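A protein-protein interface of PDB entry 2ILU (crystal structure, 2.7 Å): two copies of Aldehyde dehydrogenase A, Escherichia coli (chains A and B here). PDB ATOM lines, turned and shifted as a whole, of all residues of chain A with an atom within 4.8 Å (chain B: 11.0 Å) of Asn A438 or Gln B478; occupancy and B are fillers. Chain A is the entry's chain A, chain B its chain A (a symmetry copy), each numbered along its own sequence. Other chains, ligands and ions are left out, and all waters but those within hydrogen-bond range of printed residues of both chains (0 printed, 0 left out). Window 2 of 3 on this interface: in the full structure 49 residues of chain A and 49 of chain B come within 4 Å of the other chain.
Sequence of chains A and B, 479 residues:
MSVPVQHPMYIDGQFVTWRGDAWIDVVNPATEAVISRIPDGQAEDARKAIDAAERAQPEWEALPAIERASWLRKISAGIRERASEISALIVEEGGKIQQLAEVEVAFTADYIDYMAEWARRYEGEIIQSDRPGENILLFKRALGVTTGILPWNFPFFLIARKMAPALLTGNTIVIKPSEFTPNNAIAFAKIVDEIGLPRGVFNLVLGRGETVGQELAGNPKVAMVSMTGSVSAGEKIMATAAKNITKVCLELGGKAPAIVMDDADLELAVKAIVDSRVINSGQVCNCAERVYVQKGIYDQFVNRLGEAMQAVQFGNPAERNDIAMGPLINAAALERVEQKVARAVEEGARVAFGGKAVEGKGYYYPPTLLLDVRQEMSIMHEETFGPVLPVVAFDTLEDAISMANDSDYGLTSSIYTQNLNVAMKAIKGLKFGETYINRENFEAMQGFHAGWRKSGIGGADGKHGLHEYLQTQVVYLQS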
ATOM      1  N   LEU A 268     -19.789 -13.142  22.719  1.00  0.00           N
ATOM      2  CA  LEU A 268     -18.486 -13.135  22.076  1.00  0.00           C
ATOM      3  C   LEU A 268     -18.171 -14.458  21.353  1.00  0.00           C
ATOM      4  O   LEU A 268     -17.873 -14.439  20.159  1.00  0.00           O
ATOM      5  CB  LEU A 268     -17.408 -12.841  23.126  1.00  0.00           C
ATOM      6  CG  LEU A 268     -15.983 -12.470  22.688  1.00  0.00           C
ATOM      7  CD1 LEU A 268     -15.171 -12.093  23.926  1.00  0.00           C
ATOM      8  CD2 LEU A 268     -15.319 -13.627  21.945  1.00  0.00           C
ATOM      9  N   ILE A 415      -9.886 -20.788  22.743  1.00  0.00           N
ATOM     10  CA  ILE A 415     -10.636 -21.047  23.952  1.00  0.00           C
ATOM     11  C   ILE A 415     -11.380 -19.810  24.470  1.00  0.00           C
ATOM     12  O   ILE A 415     -10.797 -18.731  24.508  1.00  0.00           O
ATOM     13  CB  ILE A 415      -9.719 -21.593  25.058  1.00  0.00           C
ATOM     14  CG1 ILE A 415     -10.563 -22.019  26.264  1.00  0.00           C
ATOM     15  CG2 ILE A 415      -8.672 -20.546  25.429  1.00  0.00           C
ATOM     16  CD1 ILE A 415      -9.818 -22.872  27.269  1.00  0.00           C
ATOM     17  N   TYR A 416     -12.652 -19.966  24.809  1.00  0.00           N
ATOM     18  CA  TYR A 416     -13.416 -18.852  25.329  1.00  0.00           C
ATOM     19  C   TYR A 416     -13.774 -19.039  26.795  1.00  0.00           C
ATOM     20  O   TYR A 416     -14.670 -19.815  27.106  1.00  0.00           O
ATOM     21  CB  TYR A 416     -14.678 -18.646  24.503  1.00  0.00           C
ATOM     22  CG  TYR A 416     -14.386 -18.525  23.033  1.00  0.00           C
ATOM     23  CD1 TYR A 416     -14.339 -19.655  22.223  1.00  0.00           C
ATOM     24  CD2 TYR A 416     -14.106 -17.288  22.457  1.00  0.00           C
ATOM     25  CE1 TYR A 416     -14.019 -19.561  20.870  1.00  0.00           C
ATOM     26  CE2 TYR A 416     -13.782 -17.181  21.107  1.00  0.00           C
ATOM     27  CZ  TYR A 416     -13.738 -18.324  20.319  1.00  0.00           C
ATOM     28  OH  TYR A 416     -13.392 -18.244  18.988  1.00  0.00           O
ATOM     29  N   THR A 417     -13.037 -18.359  27.659  1.00  0.00           N
ATOM     30  CA  THR A 417     -13.244 -18.430  29.089  1.00  0.00           C
ATOM     31  C   THR A 417     -12.938 -17.088  29.764  1.00  0.00           C
ATOM     32  O   THR A 417     -12.753 -16.100  29.050  1.00  0.00           O
ATOM     33  CB  THR A 417     -12.341 -19.513  29.730  1.00  0.00           C
ATOM     34  OG1 THR A 417     -12.793 -19.789  31.060  1.00  0.00           O
ATOM     35  CG2 THR A 417     -10.889 -19.034  29.809  1.00  0.00           C
ATOM     36  N   TYR A 436      -6.042 -18.938  20.235  1.00  0.00           N
ATOM     37  CA  TYR A 436      -6.759 -17.702  20.421  1.00  0.00           C
ATOM     38  C   TYR A 436      -7.614 -17.695  21.694  1.00  0.00           C
ATOM     39  O   TYR A 436      -8.353 -18.653  21.935  1.00  0.00           O
ATOM     40  CB  TYR A 436      -7.617 -17.426  19.194  1.00  0.00           C
ATOM     41  CG  TYR A 436      -6.785 -17.181  17.963  1.00  0.00           C
ATOM     42  CD1 TYR A 436      -6.189 -18.235  17.278  1.00  0.00           C
ATOM     43  CD2 TYR A 436      -6.565 -15.883  17.501  1.00  0.00           C
ATOM     44  CE1 TYR A 436      -5.395 -18.003  16.155  1.00  0.00           C
ATOM     45  CE2 TYR A 436      -5.772 -15.638  16.387  1.00  0.00           C
ATOM     46  CZ  TYR A 436      -5.191 -16.698  15.716  1.00  0.00           C
ATOM     47  OH  TYR A 436      -4.406 -16.450  14.612  1.00  0.00           O
ATOM     48  N   ILE A 437      -7.479 -16.654  22.503  1.00  0.00           N
ATOM     49  CA  ILE A 437      -8.260 -16.565  23.719  1.00  0.00           C
ATOM     50  C   ILE A 437      -9.285 -15.416  23.712  1.00  0.00           C
ATOM     51  O   ILE A 437      -8.891 -14.251  23.810  1.00  0.00           O
ATOM     52  CB  ILE A 437      -7.347 -16.412  24.929  1.00  0.00           C
ATOM     53  CG1 ILE A 437      -6.434 -17.630  25.033  1.00  0.00           C
ATOM     54  CG2 ILE A 437      -8.182 -16.255  26.190  1.00  0.00           C
ATOM     55  CD1 ILE A 437      -5.436 -17.545  26.164  1.00  0.00           C
ATOM     56  N   ASN A 438     -10.563 -15.758  23.593  1.00  0.00           N
ATOM     57  CA  ASN A 438     -11.644 -14.776  23.561  1.00  0.00           C
ATOM     58  C   ASN A 438     -11.646 -13.853  22.325  1.00  0.00           C
ATOM     59  O   ASN A 438     -11.896 -12.651  22.458  1.00  0.00           O
ATOM     60  CB  ASN A 438     -11.635 -13.929  24.836  1.00  0.00           C
ATOM     61  CG  ASN A 438     -11.878 -14.756  26.081  1.00  0.00           C
ATOM     62  OD1 ASN A 438     -12.750 -15.622  26.100  1.00  0.00           O
ATOM     63  ND2 ASN A 438     -11.111 -14.488  27.131  1.00  0.00           N
ATOM     64  N   ARG A 439     -11.363 -14.430  21.160  1.00  0.00           N
ATOM     65  CA  ARG A 439     -11.354 -13.695  19.901  1.00  0.00           C
ATOM     66  C   ARG A 439     -11.315 -14.615  18.666  1.00  0.00           C
ATOM     67  O   ARG A 439     -10.980 -15.792  18.815  1.00  0.00           O
ATOM     68  CB  ARG A 439     -10.174 -12.725  19.852  1.00  0.00           C
ATOM     69  CG  ARG A 439      -8.824 -13.363  20.096  1.00  0.00           C
ATOM     70  CD  ARG A 439      -7.731 -12.617  19.339  1.00  0.00           C
ATOM     71  NE  ARG A 439      -7.923 -12.735  17.895  1.00  0.00           N
ATOM     72  CZ  ARG A 439      -7.044 -12.346  16.977  1.00  0.00           C
ATOM     73  NH1 ARG A 439      -5.893 -11.799  17.342  1.00  0.00           N
ATOM     74  NH2 ARG A 439      -7.312 -12.521  15.688  1.00  0.00           N
ATOM     75  N   ILE B 127       5.299 -10.264  21.553  1.00  0.00           N
ATOM     76  CA  ILE B 127       5.162  -9.406  20.402  1.00  0.00           C
ATOM     77  C   ILE B 127       4.043  -8.374  20.451  1.00  0.00           C
ATOM     78  O   ILE B 127       2.936  -8.702  20.882  1.00  0.00           O
ATOM     79  CB  ILE B 127       4.968 -10.270  19.164  1.00  0.00           C
ATOM     80  CG1 ILE B 127       6.083 -11.312  19.107  1.00  0.00           C
ATOM     81  CG2 ILE B 127       4.960  -9.404  17.913  1.00  0.00           C
ATOM     82  CD1 ILE B 127       5.701 -12.571  18.374  1.00  0.00           C
ATOM     83  N   GLN B 128       4.353  -7.157  20.013  1.00  0.00           N
ATOM     84  CA  GLN B 128       3.384  -6.073  19.959  1.00  0.00           C
ATOM     85  C   GLN B 128       2.250  -6.387  18.981  1.00  0.00           C
ATOM     86  O   GLN B 128       2.531  -6.729  17.842  1.00  0.00           O
ATOM     87  CB  GLN B 128       4.061  -4.772  19.501  1.00  0.00           C
ATOM     88  CG  GLN B 128       5.094  -4.194  20.453  1.00  0.00           C
ATOM     89  CD  GLN B 128       4.472  -3.644  21.728  1.00  0.00           C
ATOM     90  OE1 GLN B 128       3.591  -2.783  21.677  1.00  0.00           O
ATOM     91  NE2 GLN B 128       4.935  -4.135  22.879  1.00  0.00           N
ATOM     92  N   SER B 129       1.010  -6.291  19.421  1.00  0.00           N
ATOM     93  CA  SER B 129      -0.109  -6.545  18.533  1.00  0.00           C
ATOM     94  C   SER B 129      -0.690  -5.245  17.950  1.00  0.00           C
ATOM     95  O   SER B 129      -0.384  -4.184  18.491  1.00  0.00           O
ATOM     96  CB  SER B 129      -1.194  -7.297  19.295  1.00  0.00           C
ATOM     97  OG  SER B 129      -2.478  -7.036  18.762  1.00  0.00           O
ATOM     98  N   ASP B 130      -1.454  -5.323  16.863  1.00  0.00           N
ATOM     99  CA  ASP B 130      -2.090  -4.132  16.296  1.00  0.00           C
ATOM    100  C   ASP B 130      -3.487  -3.937  16.902  1.00  0.00           C
ATOM    101  O   ASP B 130      -4.123  -2.900  16.692  1.00  0.00           O
ATOM    102  CB  ASP B 130      -2.225  -4.235  14.769  1.00  0.00           C
ATOM    103  CG  ASP B 130      -0.880  -4.307  14.064  1.00  0.00           C
ATOM    104  OD1 ASP B 130       0.154  -4.052  14.718  1.00  0.00           O
ATOM    105  OD2 ASP B 130      -0.858  -4.613  12.854  1.00  0.00           O
ATOM    106  N   ARG B 131      -3.929  -4.947  17.641  1.00  0.00           N
ATOM    107  CA  ARG B 131      -5.223  -4.937  18.297  1.00  0.00           C
ATOM    108  C   ARG B 131      -5.212  -4.286  19.680  1.00  0.00           C
ATOM    109  O   ARG B 131      -4.491  -4.745  20.559  1.00  0.00           O
ATOM    110  CB  ARG B 131      -5.739  -6.362  18.447  1.00  0.00           C
ATOM    111  CG  ARG B 131      -6.271  -6.993  17.180  1.00  0.00           C
ATOM    112  CD  ARG B 131      -6.299  -8.506  17.344  1.00  0.00           C
ATOM    113  NE  ARG B 131      -7.270  -9.157  16.469  1.00  0.00           N
ATOM    114  CZ  ARG B 131      -8.585  -9.125  16.660  1.00  0.00           C
ATOM    115  NH1 ARG B 131      -9.093  -8.468  17.698  1.00  0.00           N
ATOM    116  NH2 ARG B 131      -9.388  -9.763  15.819  1.00  0.00           N
ATOM    117  N   PRO B 132      -6.006  -3.230  19.881  1.00  0.00           N
ATOM    118  CA  PRO B 132      -6.055  -2.554  21.180  1.00  0.00           C
ATOM    119  C   PRO B 132      -6.169  -3.531  22.387  1.00  0.00           C
ATOM    120  O   PRO B 132      -7.114  -4.328  22.450  1.00  0.00           O
ATOM    121  CB  PRO B 132      -7.282  -1.663  21.046  1.00  0.00           C
ATOM    122  CG  PRO B 132      -7.255  -1.294  19.589  1.00  0.00           C
ATOM    123  CD  PRO B 132      -6.933  -2.606  18.921  1.00  0.00           C
ATOM    124  N   GLY B 133      -5.204  -3.462  23.299  1.00  0.00           N
ATOM    125  CA  GLY B 133      -5.233  -4.305  24.481  1.00  0.00           C
ATOM    126  C   GLY B 133      -5.028  -5.793  24.268  1.00  0.00           C
ATOM    127  O   GLY B 133      -5.515  -6.609  25.052  1.00  0.00           O
ATOM    128  N   GLU B 134      -4.315  -6.160  23.211  1.00  0.00           N
ATOM    129  CA  GLU B 134      -4.064  -7.570  22.977  1.00  0.00           C
ATOM    130  C   GLU B 134      -2.597  -7.973  23.153  1.00  0.00           C
ATOM    131  O   GLU B 134      -1.713  -7.247  22.717  1.00  0.00           O
ATOM    132  CB  GLU B 134      -4.512  -7.993  21.582  1.00  0.00           C
ATOM    133  CG  GLU B 134      -4.268  -9.472  21.345  1.00  0.00           C
ATOM    134  CD  GLU B 134      -4.354  -9.866  19.891  1.00  0.00           C
ATOM    135  OE1 GLU B 134      -3.568  -9.337  19.076  1.00  0.00           O
ATOM    136  OE2 GLU B 134      -5.209 -10.714  19.562  1.00  0.00           O
ATOM    137  N   ASN B 135      -2.355  -9.103  23.796  1.00  0.00           N
ATOM    138  CA  ASN B 135      -0.993  -9.561  23.970  1.00  0.00           C
ATOM    139  C   ASN B 135      -0.664 -10.785  23.124  1.00  0.00           C
ATOM    140  O   ASN B 135      -1.444 -11.744  23.105  1.00  0.00           O
ATOM    141  CB  ASN B 135      -0.708  -9.883  25.443  1.00  0.00           C
ATOM    142  CG  ASN B 135      -0.562  -8.636  26.296  1.00  0.00           C
ATOM    143  OD1 ASN B 135       0.325  -7.812  26.062  1.00  0.00           O
ATOM    144  ND2 ASN B 135      -1.437  -8.490  27.292  1.00  0.00           N
ATOM    145  N   ILE B 136       0.440 -10.731  22.400  1.00  0.00           N
ATOM    146  CA  ILE B 136       0.836 -11.884  21.631  1.00  0.00           C
ATOM    147  C   ILE B 136       2.011 -12.573  22.308  1.00  0.00           C
ATOM    148  O   ILE B 136       3.123 -12.041  22.289  1.00  0.00           O
ATOM    149  CB  ILE B 136       1.248 -11.526  20.201  1.00  0.00           C
ATOM    150  CG1 ILE B 136       0.095 -10.835  19.478  1.00  0.00           C
ATOM    151  CG2 ILE B 136       1.643 -12.798  19.447  1.00  0.00           C
ATOM    152  CD1 ILE B 136       0.448 -10.347  18.086  1.00  0.00           C
ATOM    153  N   LEU B 137       1.745 -13.699  22.946  1.00  0.00           N
ATOM    154  CA  LEU B 137       2.804 -14.433  23.597  1.00  0.00           C
ATOM    155  C   LEU B 137       3.313 -15.571  22.718  1.00  0.00           C
ATOM    156  O   LEU B 137       2.503 -16.306  22.140  1.00  0.00           O
ATOM    157  CB  LEU B 137       2.308 -15.001  24.918  1.00  0.00           C
ATOM    158  CG  LEU B 137       1.612 -13.986  25.818  1.00  0.00           C
ATOM    159  CD1 LEU B 137       0.966 -14.744  26.975  1.00  0.00           C
ATOM    160  CD2 LEU B 137       2.596 -12.923  26.318  1.00  0.00           C
ATOM    161  N   VAL B 474       2.101 -19.742  19.558  1.00  0.00           N
ATOM    162  CA  VAL B 474       1.716 -18.344  19.597  1.00  0.00           C
ATOM    163  C   VAL B 474       0.335 -18.128  20.224  1.00  0.00           C
ATOM    164  O   VAL B 474      -0.666 -18.579  19.663  1.00  0.00           O
ATOM    165  CB  VAL B 474       1.729 -17.718  18.186  1.00  0.00           C
ATOM    166  CG1 VAL B 474       1.400 -16.256  18.272  1.00  0.00           C
ATOM    167  CG2 VAL B 474       3.096 -17.893  17.549  1.00  0.00           C
ATOM    168  N   VAL B 475       0.305 -17.468  21.374  1.00  0.00           N
ATOM    169  CA  VAL B 475      -0.948 -17.200  22.051  1.00  0.00           C
ATOM    170  C   VAL B 475      -1.457 -15.765  21.857  1.00  0.00           C
ATOM    171  O   VAL B 475      -0.734 -14.823  22.184  1.00  0.00           O
ATOM    172  CB  VAL B 475      -0.830 -17.440  23.569  1.00  0.00           C
ATOM    173  CG1 VAL B 475      -2.191 -17.239  24.234  1.00  0.00           C
ATOM    174  CG2 VAL B 475      -0.288 -18.826  23.831  1.00  0.00           C
ATOM    175  N   TYR B 476      -2.661 -15.625  21.319  1.00  0.00           N
ATOM    176  CA  TYR B 476      -3.265 -14.319  21.132  1.00  0.00           C
ATOM    177  C   TYR B 476      -4.242 -14.020  22.263  1.00  0.00           C
ATOM    178  O   TYR B 476      -5.427 -14.313  22.134  1.00  0.00           O
ATOM    179  CB  TYR B 476      -4.006 -14.238  19.795  1.00  0.00           C
ATOM    180  CG  TYR B 476      -3.115 -14.288  18.574  1.00  0.00           C
ATOM    181  CD1 TYR B 476      -2.545 -15.492  18.144  1.00  0.00           C
ATOM    182  CD2 TYR B 476      -2.846 -13.128  17.838  1.00  0.00           C
ATOM    183  CE1 TYR B 476      -1.733 -15.540  17.008  1.00  0.00           C
ATOM    184  CE2 TYR B 476      -2.036 -13.167  16.705  1.00  0.00           C
ATOM    185  CZ  TYR B 476      -1.485 -14.371  16.296  1.00  0.00           C
ATOM    186  OH  TYR B 476      -0.687 -14.410  15.174  1.00  0.00           O
ATOM    187  N   LEU B 477      -3.731 -13.473  23.356  1.00  0.00           N
ATOM    188  CA  LEU B 477      -4.552 -13.159  24.516  1.00  0.00           C
ATOM    189  C   LEU B 477      -5.303 -11.817  24.408  1.00  0.00           C
ATOM    190  O   LEU B 477      -4.771 -10.788  24.819  1.00  0.00           O
ATOM    191  CB  LEU B 477      -3.673 -13.176  25.774  1.00  0.00           C
ATOM    192  CG  LEU B 477      -4.386 -13.061  27.117  1.00  0.00           C
ATOM    193  CD1 LEU B 477      -5.584 -13.985  27.151  1.00  0.00           C
ATOM    194  CD2 LEU B 477      -3.421 -13.414  28.223  1.00  0.00           C
ATOM    195  N   GLN B 478      -6.509 -11.851  23.851  1.00  0.00           N
ATOM    196  CA  GLN B 478      -7.300 -10.640  23.696  1.00  0.00           C
ATOM    197  C   GLN B 478      -7.972 -10.173  24.996  1.00  0.00           C
ATOM    198  O   GLN B 478      -8.977 -10.766  25.396  1.00  0.00           O
ATOM    199  CB  GLN B 478      -8.389 -10.833  22.638  1.00  0.00           C
ATOM    200  CG  GLN B 478      -9.175  -9.560  22.338  1.00  0.00           C
ATOM    201  CD  GLN B 478      -8.310  -8.481  21.705  1.00  0.00           C
ATOM    202  OE1 GLN B 478      -7.844  -8.631  20.575  1.00  0.00           O
ATOM    203  NE2 GLN B 478      -8.087  -7.390  22.432  1.00  0.00           N
ATOM    204  N   SER B 479      -7.427  -9.137  25.622  1.00  0.00           N
ATOM    205  CA  SER B 479      -7.981  -8.625  26.857  1.00  0.00           C
ATOM    206  C   SER B 479      -7.987  -9.660  28.024  1.00  0.00           C
ATOM    207  O   SER B 479      -7.201  -9.481  28.985  1.00  0.00           O
ATOM    208  CB  SER B 479      -9.406  -8.105  26.588  1.00  0.00           C
ATOM    209  OG  SER B 479     -10.070  -7.710  27.772  1.00  0.00           O
ATOM    210  OXT SER B 479      -8.774 -10.651  27.917  1.00  0.00           O
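Printed residues of chain A that touch a printed residue of chain B: Tyr A436, Ile A437, Asn A438 and Arg A439.
Hydrophobic or aromatic side chains of chain A within 4 Å of the printed part of chain B: Tyr A436 and Ile A437.
Hydrophobic or aromatic side chains of chain B that line the printed part of chain A: Val B475, Tyr B476 and Leu B477.
Among the printed residues, 10 pairs touch across the chains.
Among the printed residues, merely in contact across the chains: Arg A439 with Tyr B476 (3.4 Å), Ile A437 with Leu B477 (3.6 Å), Arg A439 with Gln B478 (3.6 Å), Tyr A436 with Tyr B476 (3.7 Å), Ile A437 with Val B475 (3.8 Å) and Asn A438 with Gln B478 (3.95 Å).
No residue of chain B comes within 4 Å of Thr A417.
Of chain B, only Val B475 (3.8 Å), Tyr B476 (3.1 Å), Leu B477 (3.6 Å) and Gln B478 (3.4 Å) come within 4 Å of Ile A437.
Of chain B, only Gln B478 (3.95 Å) comes within 4 Å of Asn A438.
Of the printed residues of chain A, Arg B131 touches Arg A439 (3.1 Å).
Printed residues of chain A within 4 Å of Leu B477: Ile A437.
Gln B478 touches three residues of chain A.
The nearest residue of chain B that does not touch Asn A438 is Ser B479 (4.6 Å).
The backbone carbonyl oxygen of Leu B137 lies within hydrogen-bond range of the backbone NH of Val B475, at 2.6 Å.
The side-chain hydroxyl (OG) of Ser B129 is in hydrogen-bond range of the backbone NH (N) of Arg B131, at 2.8 Å.
O of Ile A415 is in hydrogen-bond range of N of Asn A438 (3.1 Å).
O of Thr A417 sits close to OD1 of Asn A438 (3.0 Å).
The backbone carbonyl oxygen (O) of Pro B132 lies within hydrogen-bond range of the side-chain amide nitrogen (NE2) of Gln B478.
The backbone NH of Ile A415 is in hydrogen-bond range of the backbone carbonyl oxygen of Tyr A436.
No position is printed for both chains.
O of Ile A437 lies within hydrogen-bond range of N of Gln B478 (3.4 Å).
N of Ile A437 is in hydrogen-bond range of O of Tyr B476 (3.1 Å).
The guanidinium group (NH1) of Arg A439 is in salt-bridge range of the side-chain carboxylate (OE2) of Glu B134.
The guanidinium group of Arg B131 lies close to the guanidinium group of Arg A439 (3.1 Å).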
